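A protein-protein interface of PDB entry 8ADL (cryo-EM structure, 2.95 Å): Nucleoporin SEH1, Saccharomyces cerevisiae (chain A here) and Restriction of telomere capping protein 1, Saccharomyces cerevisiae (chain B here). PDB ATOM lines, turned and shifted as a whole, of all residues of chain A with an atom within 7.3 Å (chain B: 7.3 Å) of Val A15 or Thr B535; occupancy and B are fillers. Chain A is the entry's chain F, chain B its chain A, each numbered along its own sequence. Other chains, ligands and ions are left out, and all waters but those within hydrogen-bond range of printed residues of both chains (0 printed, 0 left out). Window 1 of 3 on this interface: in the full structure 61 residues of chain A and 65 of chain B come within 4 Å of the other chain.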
ATOM      1  N   PHE A   4      14.463  -6.784  19.756  1.00  0.00           N
ATOM      2  CA  PHE A   4      15.329  -5.701  19.320  1.00  0.00           C
ATOM      3  C   PHE A   4      14.666  -4.368  19.629  1.00  0.00           C
ATOM      4  O   PHE A   4      13.438  -4.261  19.661  1.00  0.00           O
ATOM      5  CB  PHE A   4      15.634  -5.802  17.812  1.00  0.00           C
ATOM      6  CG  PHE A   4      14.418  -5.678  16.926  1.00  0.00           C
ATOM      7  CD1 PHE A   4      13.648  -6.791  16.623  1.00  0.00           C
ATOM      8  CD2 PHE A   4      14.069  -4.458  16.360  1.00  0.00           C
ATOM      9  CE1 PHE A   4      12.539  -6.686  15.803  1.00  0.00           C
ATOM     10  CE2 PHE A   4      12.960  -4.348  15.541  1.00  0.00           C
ATOM     11  CZ  PHE A   4      12.196  -5.463  15.260  1.00  0.00           C
ATOM     12  N   HIS A   8      12.183   4.188  17.167  1.00  0.00           N
ATOM     13  CA  HIS A   8      10.967   4.989  17.173  1.00  0.00           C
ATOM     14  C   HIS A   8      10.940   5.924  18.374  1.00  0.00           C
ATOM     15  O   HIS A   8      11.322   5.548  19.486  1.00  0.00           O
ATOM     16  CB  HIS A   8       9.735   4.086  17.204  1.00  0.00           C
ATOM     17  CG  HIS A   8       9.407   3.453  15.890  1.00  0.00           C
ATOM     18  ND1 HIS A   8       9.249   4.180  14.731  1.00  0.00           N
ATOM     19  CD2 HIS A   8       9.199   2.157  15.552  1.00  0.00           C
ATOM     20  CE1 HIS A   8       8.955   3.362  13.736  1.00  0.00           C
ATOM     21  NE2 HIS A   8       8.922   2.128  14.208  1.00  0.00           N
ATOM     22  N   VAL A  12       4.555   2.446  18.795  1.00  0.00           N
ATOM     23  CA  VAL A  12       4.423   1.677  17.563  1.00  0.00           C
ATOM     24  C   VAL A  12       3.001   1.140  17.482  1.00  0.00           C
ATOM     25  O   VAL A  12       2.527   0.472  18.409  1.00  0.00           O
ATOM     26  CB  VAL A  12       5.449   0.534  17.513  1.00  0.00           C
ATOM     27  CG1 VAL A  12       5.528  -0.039  16.111  1.00  0.00           C
ATOM     28  CG2 VAL A  12       6.810   1.024  17.976  1.00  0.00           C
ATOM     29  N   HIS A  13       2.315   1.430  16.377  1.00  0.00           N
ATOM     30  CA  HIS A  13       0.884   1.172  16.269  1.00  0.00           C
ATOM     31  C   HIS A  13       0.552  -0.122  15.539  1.00  0.00           C
ATOM     32  O   HIS A  13      -0.212  -0.942  16.057  1.00  0.00           O
ATOM     33  CB  HIS A  13       0.194   2.340  15.557  1.00  0.00           C
ATOM     34  CG  HIS A  13       0.045   3.562  16.405  1.00  0.00           C
ATOM     35  ND1 HIS A  13      -0.060   3.508  17.778  1.00  0.00           N
ATOM     36  CD2 HIS A  13      -0.025   4.873  16.074  1.00  0.00           C
ATOM     37  CE1 HIS A  13      -0.182   4.732  18.257  1.00  0.00           C
ATOM     38  NE2 HIS A  13      -0.165   5.580  17.244  1.00  0.00           N
ATOM     39  N   ASP A  14       1.104  -0.332  14.346  1.00  0.00           N
ATOM     40  CA  ASP A  14       0.824  -1.533  13.571  1.00  0.00           C
ATOM     41  C   ASP A  14       2.109  -2.116  13.008  1.00  0.00           C
ATOM     42  O   ASP A  14       2.892  -1.406  12.368  1.00  0.00           O
ATOM     43  CB  ASP A  14      -0.160  -1.225  12.439  1.00  0.00           C
ATOM     44  CG  ASP A  14      -0.821  -2.468  11.887  1.00  0.00           C
ATOM     45  OD1 ASP A  14      -1.556  -3.138  12.642  1.00  0.00           O
ATOM     46  OD2 ASP A  14      -0.617  -2.768  10.694  1.00  0.00           O
ATOM     47  N   VAL A  15       2.321  -3.406  13.254  1.00  0.00           N
ATOM     48  CA  VAL A  15       3.507  -4.128  12.815  1.00  0.00           C
ATOM     49  C   VAL A  15       3.044  -5.289  11.947  1.00  0.00           C
ATOM     50  O   VAL A  15       2.208  -6.090  12.379  1.00  0.00           O
ATOM     51  CB  VAL A  15       4.337  -4.634  14.008  1.00  0.00           C
ATOM     52  CG1 VAL A  15       5.498  -5.449  13.521  1.00  0.00           C
ATOM     53  CG2 VAL A  15       4.816  -3.471  14.854  1.00  0.00           C
ATOM     54  N   VAL A  16       3.575  -5.379  10.727  1.00  0.00           N
ATOM     55  CA  VAL A  16       3.088  -6.335   9.735  1.00  0.00           C
ATOM     56  C   VAL A  16       4.277  -6.983   9.036  1.00  0.00           C
ATOM     57  O   VAL A  16       5.162  -6.291   8.524  1.00  0.00           O
ATOM     58  CB  VAL A  16       2.138  -5.658   8.723  1.00  0.00           C
ATOM     59  CG1 VAL A  16       1.961  -6.497   7.484  1.00  0.00           C
ATOM     60  CG2 VAL A  16       0.782  -5.427   9.354  1.00  0.00           C
ATOM     61  N   TYR A  17       4.292  -8.315   9.028  1.00  0.00           N
ATOM     62  CA  TYR A  17       5.224  -9.124   8.253  1.00  0.00           C
ATOM     63  C   TYR A  17       5.086  -8.954   6.745  1.00  0.00           C
ATOM     64  O   TYR A  17       4.040  -8.579   6.217  1.00  0.00           O
ATOM     65  CB  TYR A  17       4.993 -10.596   8.546  1.00  0.00           C
ATOM     66  CG  TYR A  17       5.635 -11.150   9.774  1.00  0.00           C
ATOM     67  CD1 TYR A  17       6.806 -10.613  10.295  1.00  0.00           C
ATOM     68  CD2 TYR A  17       5.056 -12.217  10.420  1.00  0.00           C
ATOM     69  CE1 TYR A  17       7.388 -11.165  11.421  1.00  0.00           C
ATOM     70  CE2 TYR A  17       5.605 -12.735  11.534  1.00  0.00           C
ATOM     71  CZ  TYR A  17       6.767 -12.235  12.028  1.00  0.00           C
ATOM     72  OH  TYR A  17       7.268 -12.850  13.140  1.00  0.00           O
ATOM     73  N   VAL A  24      10.168  -6.974   8.514  1.00  0.00           N
ATOM     74  CA  VAL A  24       9.196  -6.456   9.471  1.00  0.00           C
ATOM     75  C   VAL A  24       9.076  -4.958   9.242  1.00  0.00           C
ATOM     76  O   VAL A  24      10.070  -4.231   9.356  1.00  0.00           O
ATOM     77  CB  VAL A  24       9.611  -6.750  10.922  1.00  0.00           C
ATOM     78  CG1 VAL A  24       8.752  -5.970  11.889  1.00  0.00           C
ATOM     79  CG2 VAL A  24       9.519  -8.233  11.212  1.00  0.00           C
ATOM     80  N   ALA A  25       7.868  -4.492   8.935  1.00  0.00           N
ATOM     81  CA  ALA A  25       7.591  -3.070   8.776  1.00  0.00           C
ATOM     82  C   ALA A  25       6.803  -2.577   9.979  1.00  0.00           C
ATOM     83  O   ALA A  25       5.682  -3.037  10.222  1.00  0.00           O
ATOM     84  CB  ALA A  25       6.824  -2.792   7.485  1.00  0.00           C
ATOM     85  N   THR A  26       7.383  -1.639  10.718  1.00  0.00           N
ATOM     86  CA  THR A  26       6.766  -1.064  11.905  1.00  0.00           C
ATOM     87  C   THR A  26       6.388   0.381  11.614  1.00  0.00           C
ATOM     88  O   THR A  26       7.265   1.212  11.349  1.00  0.00           O
ATOM     89  CB  THR A  26       7.712  -1.133  13.103  1.00  0.00           C
ATOM     90  OG1 THR A  26       8.883  -0.353  12.832  1.00  0.00           O
ATOM     91  CG2 THR A  26       8.128  -2.567  13.369  1.00  0.00           C
ATOM     92  N   CYS A  27       5.095   0.680  11.667  1.00  0.00           N
ATOM     93  CA  CYS A  27       4.617   2.046  11.531  1.00  0.00           C
ATOM     94  C   CYS A  27       4.292   2.593  12.915  1.00  0.00           C
ATOM     95  O   CYS A  27       3.810   1.864  13.787  1.00  0.00           O
ATOM     96  CB  CYS A  27       3.396   2.120  10.607  1.00  0.00           C
ATOM     97  SG  CYS A  27       1.800   1.694  11.334  1.00  0.00           S
ATOM     98  N   VAL A  59      -1.491   4.629  11.463  1.00  0.00           N
ATOM     99  CA  VAL A  59      -2.260   3.703  12.288  1.00  0.00           C
ATOM    100  C   VAL A  59      -2.401   2.323  11.666  1.00  0.00           C
ATOM    101  O   VAL A  59      -2.834   1.392  12.364  1.00  0.00           O
ATOM    102  CB  VAL A  59      -3.655   4.271  12.623  1.00  0.00           C
ATOM    103  CG1 VAL A  59      -3.523   5.529  13.460  1.00  0.00           C
ATOM    104  CG2 VAL A  59      -4.418   4.559  11.351  1.00  0.00           C
ATOM    105  N   ALA A  60      -2.055   2.153  10.391  1.00  0.00           N
ATOM    106  CA  ALA A  60      -2.167   0.852   9.751  1.00  0.00           C
ATOM    107  C   ALA A  60      -1.086   0.718   8.690  1.00  0.00           C
ATOM    108  O   ALA A  60      -0.610   1.712   8.136  1.00  0.00           O
ATOM    109  CB  ALA A  60      -3.551   0.645   9.127  1.00  0.00           C
ATOM    110  N   ILE A  61      -0.712  -0.529   8.410  1.00  0.00           N
ATOM    111  CA  ILE A  61       0.281  -0.846   7.393  1.00  0.00           C
ATOM    112  C   ILE A  61      -0.003  -2.256   6.891  1.00  0.00           C
ATOM    113  O   ILE A  61      -0.625  -3.064   7.586  1.00  0.00           O
ATOM    114  CB  ILE A  61       1.725  -0.690   7.938  1.00  0.00           C
ATOM    115  CG1 ILE A  61       2.717  -0.431   6.803  1.00  0.00           C
ATOM    116  CG2 ILE A  61       2.150  -1.902   8.754  1.00  0.00           C
ATOM    117  CD1 ILE A  61       4.123  -0.147   7.282  1.00  0.00           C
ATOM    118  N   TRP A  63       1.742  -5.212   3.776  1.00  0.00           N
ATOM    119  CA  TRP A  63       2.562  -5.566   2.628  1.00  0.00           C
ATOM    120  C   TRP A  63       1.687  -6.114   1.509  1.00  0.00           C
ATOM    121  O   TRP A  63       0.656  -6.746   1.751  1.00  0.00           O
ATOM    122  CB  TRP A  63       3.614  -6.613   2.998  1.00  0.00           C
ATOM    123  CG  TRP A  63       4.715  -6.124   3.876  1.00  0.00           C
ATOM    124  CD1 TRP A  63       4.622  -5.771   5.187  1.00  0.00           C
ATOM    125  CD2 TRP A  63       6.093  -5.975   3.517  1.00  0.00           C
ATOM    126  NE1 TRP A  63       5.852  -5.400   5.665  1.00  0.00           N
ATOM    127  CE2 TRP A  63       6.773  -5.513   4.659  1.00  0.00           C
ATOM    128  CE3 TRP A  63       6.817  -6.179   2.338  1.00  0.00           C
ATOM    129  CZ2 TRP A  63       8.140  -5.249   4.659  1.00  0.00           C
ATOM    130  CZ3 TRP A  63       8.174  -5.916   2.339  1.00  0.00           C
ATOM    131  CH2 TRP A  63       8.822  -5.457   3.492  1.00  0.00           C
ATOM    132  N   LYS A 115      -5.847  -2.646   4.082  1.00  0.00           N
ATOM    133  CA  LYS A 115      -5.589  -4.071   3.920  1.00  0.00           C
ATOM    134  C   LYS A 115      -5.526  -4.411   2.441  1.00  0.00           C
ATOM    135  O   LYS A 115      -6.377  -3.967   1.665  1.00  0.00           O
ATOM    136  CB  LYS A 115      -6.673  -4.917   4.603  1.00  0.00           C
ATOM    137  CG  LYS A 115      -6.400  -5.242   6.061  1.00  0.00           C
ATOM    138  CD  LYS A 115      -5.181  -6.136   6.202  1.00  0.00           C
ATOM    139  CE  LYS A 115      -4.901  -6.459   7.661  1.00  0.00           C
ATOM    140  NZ  LYS A 115      -3.611  -7.182   7.828  1.00  0.00           N
ATOM    141  N   SER A 309      -5.342  -6.147  19.743  1.00  0.00           N
ATOM    142  CA  SER A 309      -5.021  -6.878  18.525  1.00  0.00           C
ATOM    143  C   SER A 309      -5.308  -8.363  18.682  1.00  0.00           C
ATOM    144  O   SER A 309      -5.065  -8.940  19.743  1.00  0.00           O
ATOM    145  CB  SER A 309      -3.557  -6.680  18.133  1.00  0.00           C
ATOM    146  OG  SER A 309      -3.240  -7.407  16.958  1.00  0.00           O
ATOM    147  N   VAL A 310      -5.827  -8.972  17.612  1.00  0.00           N
ATOM    148  CA  VAL A 310      -5.929 -10.421  17.487  1.00  0.00           C
ATOM    149  C   VAL A 310      -5.416 -10.824  16.109  1.00  0.00           C
ATOM    150  O   VAL A 310      -5.570 -10.087  15.129  1.00  0.00           O
ATOM    151  CB  VAL A 310      -7.371 -10.939  17.705  1.00  0.00           C
ATOM    152  CG1 VAL A 310      -7.765 -10.829  19.169  1.00  0.00           C
ATOM    153  CG2 VAL A 310      -8.353 -10.172  16.840  1.00  0.00           C
ATOM    154  N   SER A 311      -4.793 -11.999  16.040  1.00  0.00           N
ATOM    155  CA  SER A 311      -4.211 -12.481  14.793  1.00  0.00           C
ATOM    156  C   SER A 311      -4.061 -13.991  14.850  1.00  0.00           C
ATOM    157  O   SER A 311      -3.444 -14.517  15.782  1.00  0.00           O
ATOM    158  CB  SER A 311      -2.854 -11.833  14.525  1.00  0.00           C
ATOM    159  OG  SER A 311      -2.270 -12.346  13.340  1.00  0.00           O
ATOM    160  N   TRP A 312      -4.614 -14.680  13.857  1.00  0.00           N
ATOM    161  CA  TRP A 312      -4.440 -16.118  13.750  1.00  0.00           C
ATOM    162  C   TRP A 312      -3.035 -16.449  13.253  1.00  0.00           C
ATOM    163  O   TRP A 312      -2.282 -15.583  12.803  1.00  0.00           O
ATOM    164  CB  TRP A 312      -5.482 -16.710  12.805  1.00  0.00           C
ATOM    165  CG  TRP A 312      -6.884 -16.559  13.284  1.00  0.00           C
ATOM    166  CD1 TRP A 312      -7.783 -15.615  12.890  1.00  0.00           C
ATOM    167  CD2 TRP A 312      -7.561 -17.390  14.230  1.00  0.00           C
ATOM    168  NE1 TRP A 312      -8.977 -15.800  13.541  1.00  0.00           N
ATOM    169  CE2 TRP A 312      -8.867 -16.884  14.370  1.00  0.00           C
ATOM    170  CE3 TRP A 312      -7.189 -18.512  14.978  1.00  0.00           C
ATOM    171  CZ2 TRP A 312      -9.803 -17.460  15.225  1.00  0.00           C
ATOM    172  CZ3 TRP A 312      -8.119 -19.081  15.826  1.00  0.00           C
ATOM    173  CH2 TRP A 312      -9.409 -18.555  15.943  1.00  0.00           C
ATOM    174  N   ASN A 313      -2.685 -17.728  13.335  1.00  0.00           N
ATOM    175  CA  ASN A 313      -1.496 -18.235  12.671  1.00  0.00           C
ATOM    176  C   ASN A 313      -1.884 -18.744  11.285  1.00  0.00           C
ATOM    177  O   ASN A 313      -2.999 -18.516  10.806  1.00  0.00           O
ATOM    178  CB  ASN A 313      -0.824 -19.312  13.520  1.00  0.00           C
ATOM    179  CG  ASN A 313      -1.721 -20.502  13.774  1.00  0.00           C
ATOM    180  OD1 ASN A 313      -2.947 -20.399  13.714  1.00  0.00           O
ATOM    181  ND2 ASN A 313      -1.114 -21.646  14.062  1.00  0.00           N
ATOM    182  N   SER A 320      -3.386 -15.316  18.659  1.00  0.00           N
ATOM    183  CA  SER A 320      -2.764 -14.383  19.582  1.00  0.00           C
ATOM    184  C   SER A 320      -3.747 -13.289  19.981  1.00  0.00           C
ATOM    185  O   SER A 320      -4.714 -12.997  19.273  1.00  0.00           O
ATOM    186  CB  SER A 320      -1.518 -13.756  18.966  1.00  0.00           C
ATOM    187  OG  SER A 320      -0.457 -14.690  18.894  1.00  0.00           O
ATOM    188  N   ASN B 532      -0.791  -2.340  21.266  1.00  0.00           N
ATOM    189  CA  ASN B 532      -0.043  -3.571  21.080  1.00  0.00           C
ATOM    190  C   ASN B 532      -0.543  -4.267  19.822  1.00  0.00           C
ATOM    191  O   ASN B 532      -1.680  -4.068  19.389  1.00  0.00           O
ATOM    192  CB  ASN B 532      -0.167  -4.482  22.307  1.00  0.00           C
ATOM    193  CG  ASN B 532       1.139  -5.168  22.661  1.00  0.00           C
ATOM    194  OD1 ASN B 532       1.973  -5.427  21.795  1.00  0.00           O
ATOM    195  ND2 ASN B 532       1.323  -5.463  23.942  1.00  0.00           N
ATOM    196  N   THR B 533       0.325  -5.088  19.234  1.00  0.00           N
ATOM    197  CA  THR B 533      -0.025  -5.816  18.023  1.00  0.00           C
ATOM    198  C   THR B 533       0.678  -7.166  18.020  1.00  0.00           C
ATOM    199  O   THR B 533       1.735  -7.333  18.631  1.00  0.00           O
ATOM    200  CB  THR B 533       0.322  -5.013  16.763  1.00  0.00           C
ATOM    201  OG1 THR B 533      -0.051  -5.761  15.598  1.00  0.00           O
ATOM    202  CG2 THR B 533       1.803  -4.687  16.719  1.00  0.00           C
ATOM    203  N   THR B 534       0.062  -8.140  17.346  1.00  0.00           N
ATOM    204  CA  THR B 534       0.624  -9.479  17.205  1.00  0.00           C
ATOM    205  C   THR B 534       0.474  -9.964  15.772  1.00  0.00           C
ATOM    206  O   THR B 534      -0.538  -9.696  15.122  1.00  0.00           O
ATOM    207  CB  THR B 534      -0.047 -10.495  18.143  1.00  0.00           C
ATOM    208  OG1 THR B 534      -1.463 -10.499  17.923  1.00  0.00           O
ATOM    209  CG2 THR B 534       0.262 -10.206  19.609  1.00  0.00           C
ATOM    210  N   THR B 535       1.507 -10.651  15.279  1.00  0.00           N
ATOM    211  CA  THR B 535       1.499 -11.335  13.989  1.00  0.00           C
ATOM    212  C   THR B 535       2.209 -12.674  14.138  1.00  0.00           C
ATOM    213  O   THR B 535       3.056 -12.852  15.015  1.00  0.00           O
ATOM    214  CB  THR B 535       2.178 -10.521  12.871  1.00  0.00           C
ATOM    215  OG1 THR B 535       3.522 -10.197  13.251  1.00  0.00           O
ATOM    216  CG2 THR B 535       1.400  -9.256  12.528  1.00  0.00           C
ATOM    217  N   TRP B 536       1.867 -13.618  13.260  1.00  0.00           N
ATOM    218  CA  TRP B 536       2.503 -14.928  13.233  1.00  0.00           C
ATOM    219  C   TRP B 536       3.260 -15.124  11.926  1.00  0.00           C
ATOM    220  O   TRP B 536       2.843 -14.640  10.870  1.00  0.00           O
ATOM    221  CB  TRP B 536       1.482 -16.063  13.385  1.00  0.00           C
ATOM    222  CG  TRP B 536       0.865 -16.177  14.738  1.00  0.00           C
ATOM    223  CD1 TRP B 536      -0.057 -15.342  15.293  1.00  0.00           C
ATOM    224  CD2 TRP B 536       1.130 -17.189  15.715  1.00  0.00           C
ATOM    225  NE1 TRP B 536      -0.387 -15.775  16.552  1.00  0.00           N
ATOM    226  CE2 TRP B 536       0.330 -16.906  16.835  1.00  0.00           C
ATOM    227  CE3 TRP B 536       1.967 -18.308  15.748  1.00  0.00           C
ATOM    228  CZ2 TRP B 536       0.341 -17.700  17.979  1.00  0.00           C
ATOM    229  CZ3 TRP B 536       1.977 -19.093  16.882  1.00  0.00           C
ATOM    230  CH2 TRP B 536       1.171 -18.786  17.983  1.00  0.00           C
ATOM    231  N   ARG B 537       4.384 -15.840  12.007  1.00  0.00           N
ATOM    232  CA  ARG B 537       5.215 -16.112  10.839  1.00  0.00           C
ATOM    233  C   ARG B 537       4.977 -17.480  10.229  1.00  0.00           C
ATOM    234  O   ARG B 537       4.984 -17.614   9.001  1.00  0.00           O
ATOM    235  CB  ARG B 537       6.700 -15.996  11.207  1.00  0.00           C
ATOM    236  CG  ARG B 537       7.624 -15.900  10.008  1.00  0.00           C
ATOM    237  CD  ARG B 537       9.083 -16.068  10.395  1.00  0.00           C
ATOM    238  NE  ARG B 537       9.925 -16.264   9.219  1.00  0.00           N
ATOM    239  CZ  ARG B 537      11.237 -16.450   9.256  1.00  0.00           C
ATOM    240  NH1 ARG B 537      11.898 -16.487  10.401  1.00  0.00           N
ATOM    241  NH2 ARG B 537      11.902 -16.602   8.115  1.00  0.00           N
ATOM    242  N   ASP B 538       4.754 -18.496  11.050  1.00  0.00           N
ATOM    243  CA  ASP B 538       4.648 -19.846  10.528  1.00  0.00           C
ATOM    244  C   ASP B 538       3.713 -20.650  11.422  1.00  0.00           C
ATOM    245  O   ASP B 538       2.950 -20.085  12.214  1.00  0.00           O
ATOM    246  CB  ASP B 538       6.054 -20.454  10.389  1.00  0.00           C
ATOM    247  CG  ASP B 538       6.857 -20.373  11.670  1.00  0.00           C
ATOM    248  OD1 ASP B 538       6.386 -19.749  12.644  1.00  0.00           O
ATOM    249  OD2 ASP B 538       7.969 -20.939  11.699  1.00  0.00           O
ATOM    250  N   GLY B 543       8.385 -17.095  14.763  1.00  0.00           N
ATOM    251  CA  GLY B 543       8.369 -15.658  14.939  1.00  0.00           C
ATOM    252  C   GLY B 543       7.030 -15.104  15.378  1.00  0.00           C
ATOM    253  O   GLY B 543       6.062 -15.116  14.612  1.00  0.00           O
ATOM    254  N   LEU B 544       6.963 -14.616  16.613  1.00  0.00           N
ATOM    255  CA  LEU B 544       5.755 -14.023  17.166  1.00  0.00           C
ATOM    256  C   LEU B 544       6.123 -12.673  17.760  1.00  0.00           C
ATOM    257  O   LEU B 544       7.081 -12.576  18.532  1.00  0.00           O
ATOM    258  CB  LEU B 544       5.137 -14.933  18.234  1.00  0.00           C
ATOM    259  CG  LEU B 544       3.875 -14.457  18.951  1.00  0.00           C
ATOM    260  CD1 LEU B 544       2.734 -14.265  17.973  1.00  0.00           C
ATOM    261  CD2 LEU B 544       3.486 -15.442  20.040  1.00  0.00           C
ATOM    262  N   LEU B 545       5.369 -11.637  17.404  1.00  0.00           N
ATOM    263  CA  LEU B 545       5.734 -10.267  17.739  1.00  0.00           C
ATOM    264  C   LEU B 545       4.751  -9.599  18.686  1.00  0.00           C
ATOM    265  O   LEU B 545       3.570  -9.947  18.758  1.00  0.00           O
ATOM    266  CB  LEU B 545       5.911  -9.398  16.487  1.00  0.00           C
ATOM    267  CG  LEU B 545       7.310  -9.386  15.859  1.00  0.00           C
ATOM    268  CD1 LEU B 545       7.719 -10.688  15.304  1.00  0.00           C
ATOM    269  CD2 LEU B 545       7.345  -8.360  14.745  1.00  0.00           C
ATOM    270  N   SER B 546       5.292  -8.624  19.409  1.00  0.00           N
ATOM    271  CA  SER B 546       4.550  -7.689  20.233  1.00  0.00           C
ATOM    272  C   SER B 546       5.288  -6.362  20.157  1.00  0.00           C
ATOM    273  O   SER B 546       6.296  -6.232  19.457  1.00  0.00           O
ATOM    274  CB  SER B 546       4.425  -8.193  21.672  1.00  0.00           C
ATOM    275  OG  SER B 546       3.916  -9.513  21.701  1.00  0.00           O
ATOM    276  N   VAL B 547       4.789  -5.369  20.883  1.00  0.00           N
ATOM    277  CA  VAL B 547       5.560  -4.164  21.163  1.00  0.00           C
ATOM    278  C   VAL B 547       5.537  -3.919  22.665  1.00  0.00           C
ATOM    279  O   VAL B 547       4.471  -3.928  23.292  1.00  0.00           O
ATOM    280  CB  VAL B 547       5.049  -2.938  20.373  1.00  0.00           C
ATOM    281  CG1 VAL B 547       5.448  -3.052  18.912  1.00  0.00           C
ATOM    282  CG2 VAL B 547       3.542  -2.804  20.460  1.00  0.00           C
ATOM    283  N   ILE B 660      10.353  -4.216  20.142  1.00  0.00           N
ATOM    284  CA  ILE B 660       9.590  -5.259  19.464  1.00  0.00           C
ATOM    285  C   ILE B 660      10.083  -6.614  19.954  1.00  0.00           C
ATOM    286  O   ILE B 660      11.275  -6.923  19.867  1.00  0.00           O
ATOM    287  CB  ILE B 660       9.700  -5.146  17.936  1.00  0.00           C
ATOM    288  CG1 ILE B 660       9.034  -3.867  17.406  1.00  0.00           C
ATOM    289  CG2 ILE B 660       9.096  -6.360  17.272  1.00  0.00           C
ATOM    290  CD1 ILE B 660       9.939  -2.661  17.296  1.00  0.00           C
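The indole nitrogen of Trp B536 lies within hydrogen-bond range of the backbone carbonyl oxygen of Ser A311 (3.4 Å). The side-chain hydroxyl of Ser A320 is in hydrogen-bond range of the indole nitrogen of Trp B536, 2.6 Å away. The side-chain hydroxyl (OG) of Ser A309 sits at hydrogen-bond distance from the backbone NH (N) of Thr B534 (3.4 Å). O of Phe A4 sits at hydrogen-bond distance from N of Ile B660. O of Gly B543 is in hydrogen-bond range of OH of Tyr A17 (3.0 Å).
N of Ser A320 is in hydrogen-bond range of O of Ser A311. N of Arg B537 sits at hydrogen-bond distance from O of Gly B543 (3.2 Å). The side-chain amide oxygen of Asn B532 lies within hydrogen-bond range of the backbone NH of Val B547, at 3.0 Å.
Leu B545 touches Val A15. Tyr A17 touches Thr B535 (CE2 to OG1, 3.7 Å). Leu B545 touches Tyr A17 (CD1 to OH, 3.1 Å). Val A24 touches Leu B545. Ser A309 touches Asn B532 (CB to O, 3.5 Å). OG of Ser A311 touches CA of Thr B535, at 3.96 Å. Trp B536 touches Trp A312. CD2 of Trp B536 touches CB of Asn A313, 3.6 Å away. Ser A320 touches Thr B534. Ser A320 touches Leu B544.
Printed residues of chain B within 4 Å of Phe A4: Ile B660. Printed residues of chain A within 4 Å of Asn B532: Ser A309 (3.5 Å). Of the printed residues of chain A, Thr B533 touches Val A15 (3.7 Å) and Ser A309 (3.6 Å). Printed residues of chain A within 4 Å of Thr B535: Val A15 (3.3 Å), Tyr A17 (3.7 Å) and Ser A311 (3.96 Å). Of the printed residues of chain A, Ile B660 touches Phe A4 (3.1 Å). The nearest residue of chain A that does not touch Thr B535 is Val A16 (4.4 Å). The nearest printed residue of chain A that does not touch Thr B533 is His A13 (4.2 Å).
Of the 23 printed residues of chain A, 10 touch a printed residue of chain B. Hydrophobic or aromatic side chains of chain A within 4 Å of the printed part of chain B: Phe A4, Val A12, Val A15, Tyr A17 and Val A24. Printed residues of chain B that touch a printed residue of chain A: Asn B532, Thr B533, Thr B534, Thr B535, Trp B536, Arg B537, Gly B543, Leu B544, Leu B545, Val B547 and Ile B660. Hydrophobic or aromatic side chains of chain B that line the printed part of chain A: Trp B536, Leu B544, Leu B545, Val B547 and Ile B660. Among the printed residues, no Asp or Glu carboxylate lies within 4 Å of a Lys or Arg side-chain nitrogen of the other chain.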
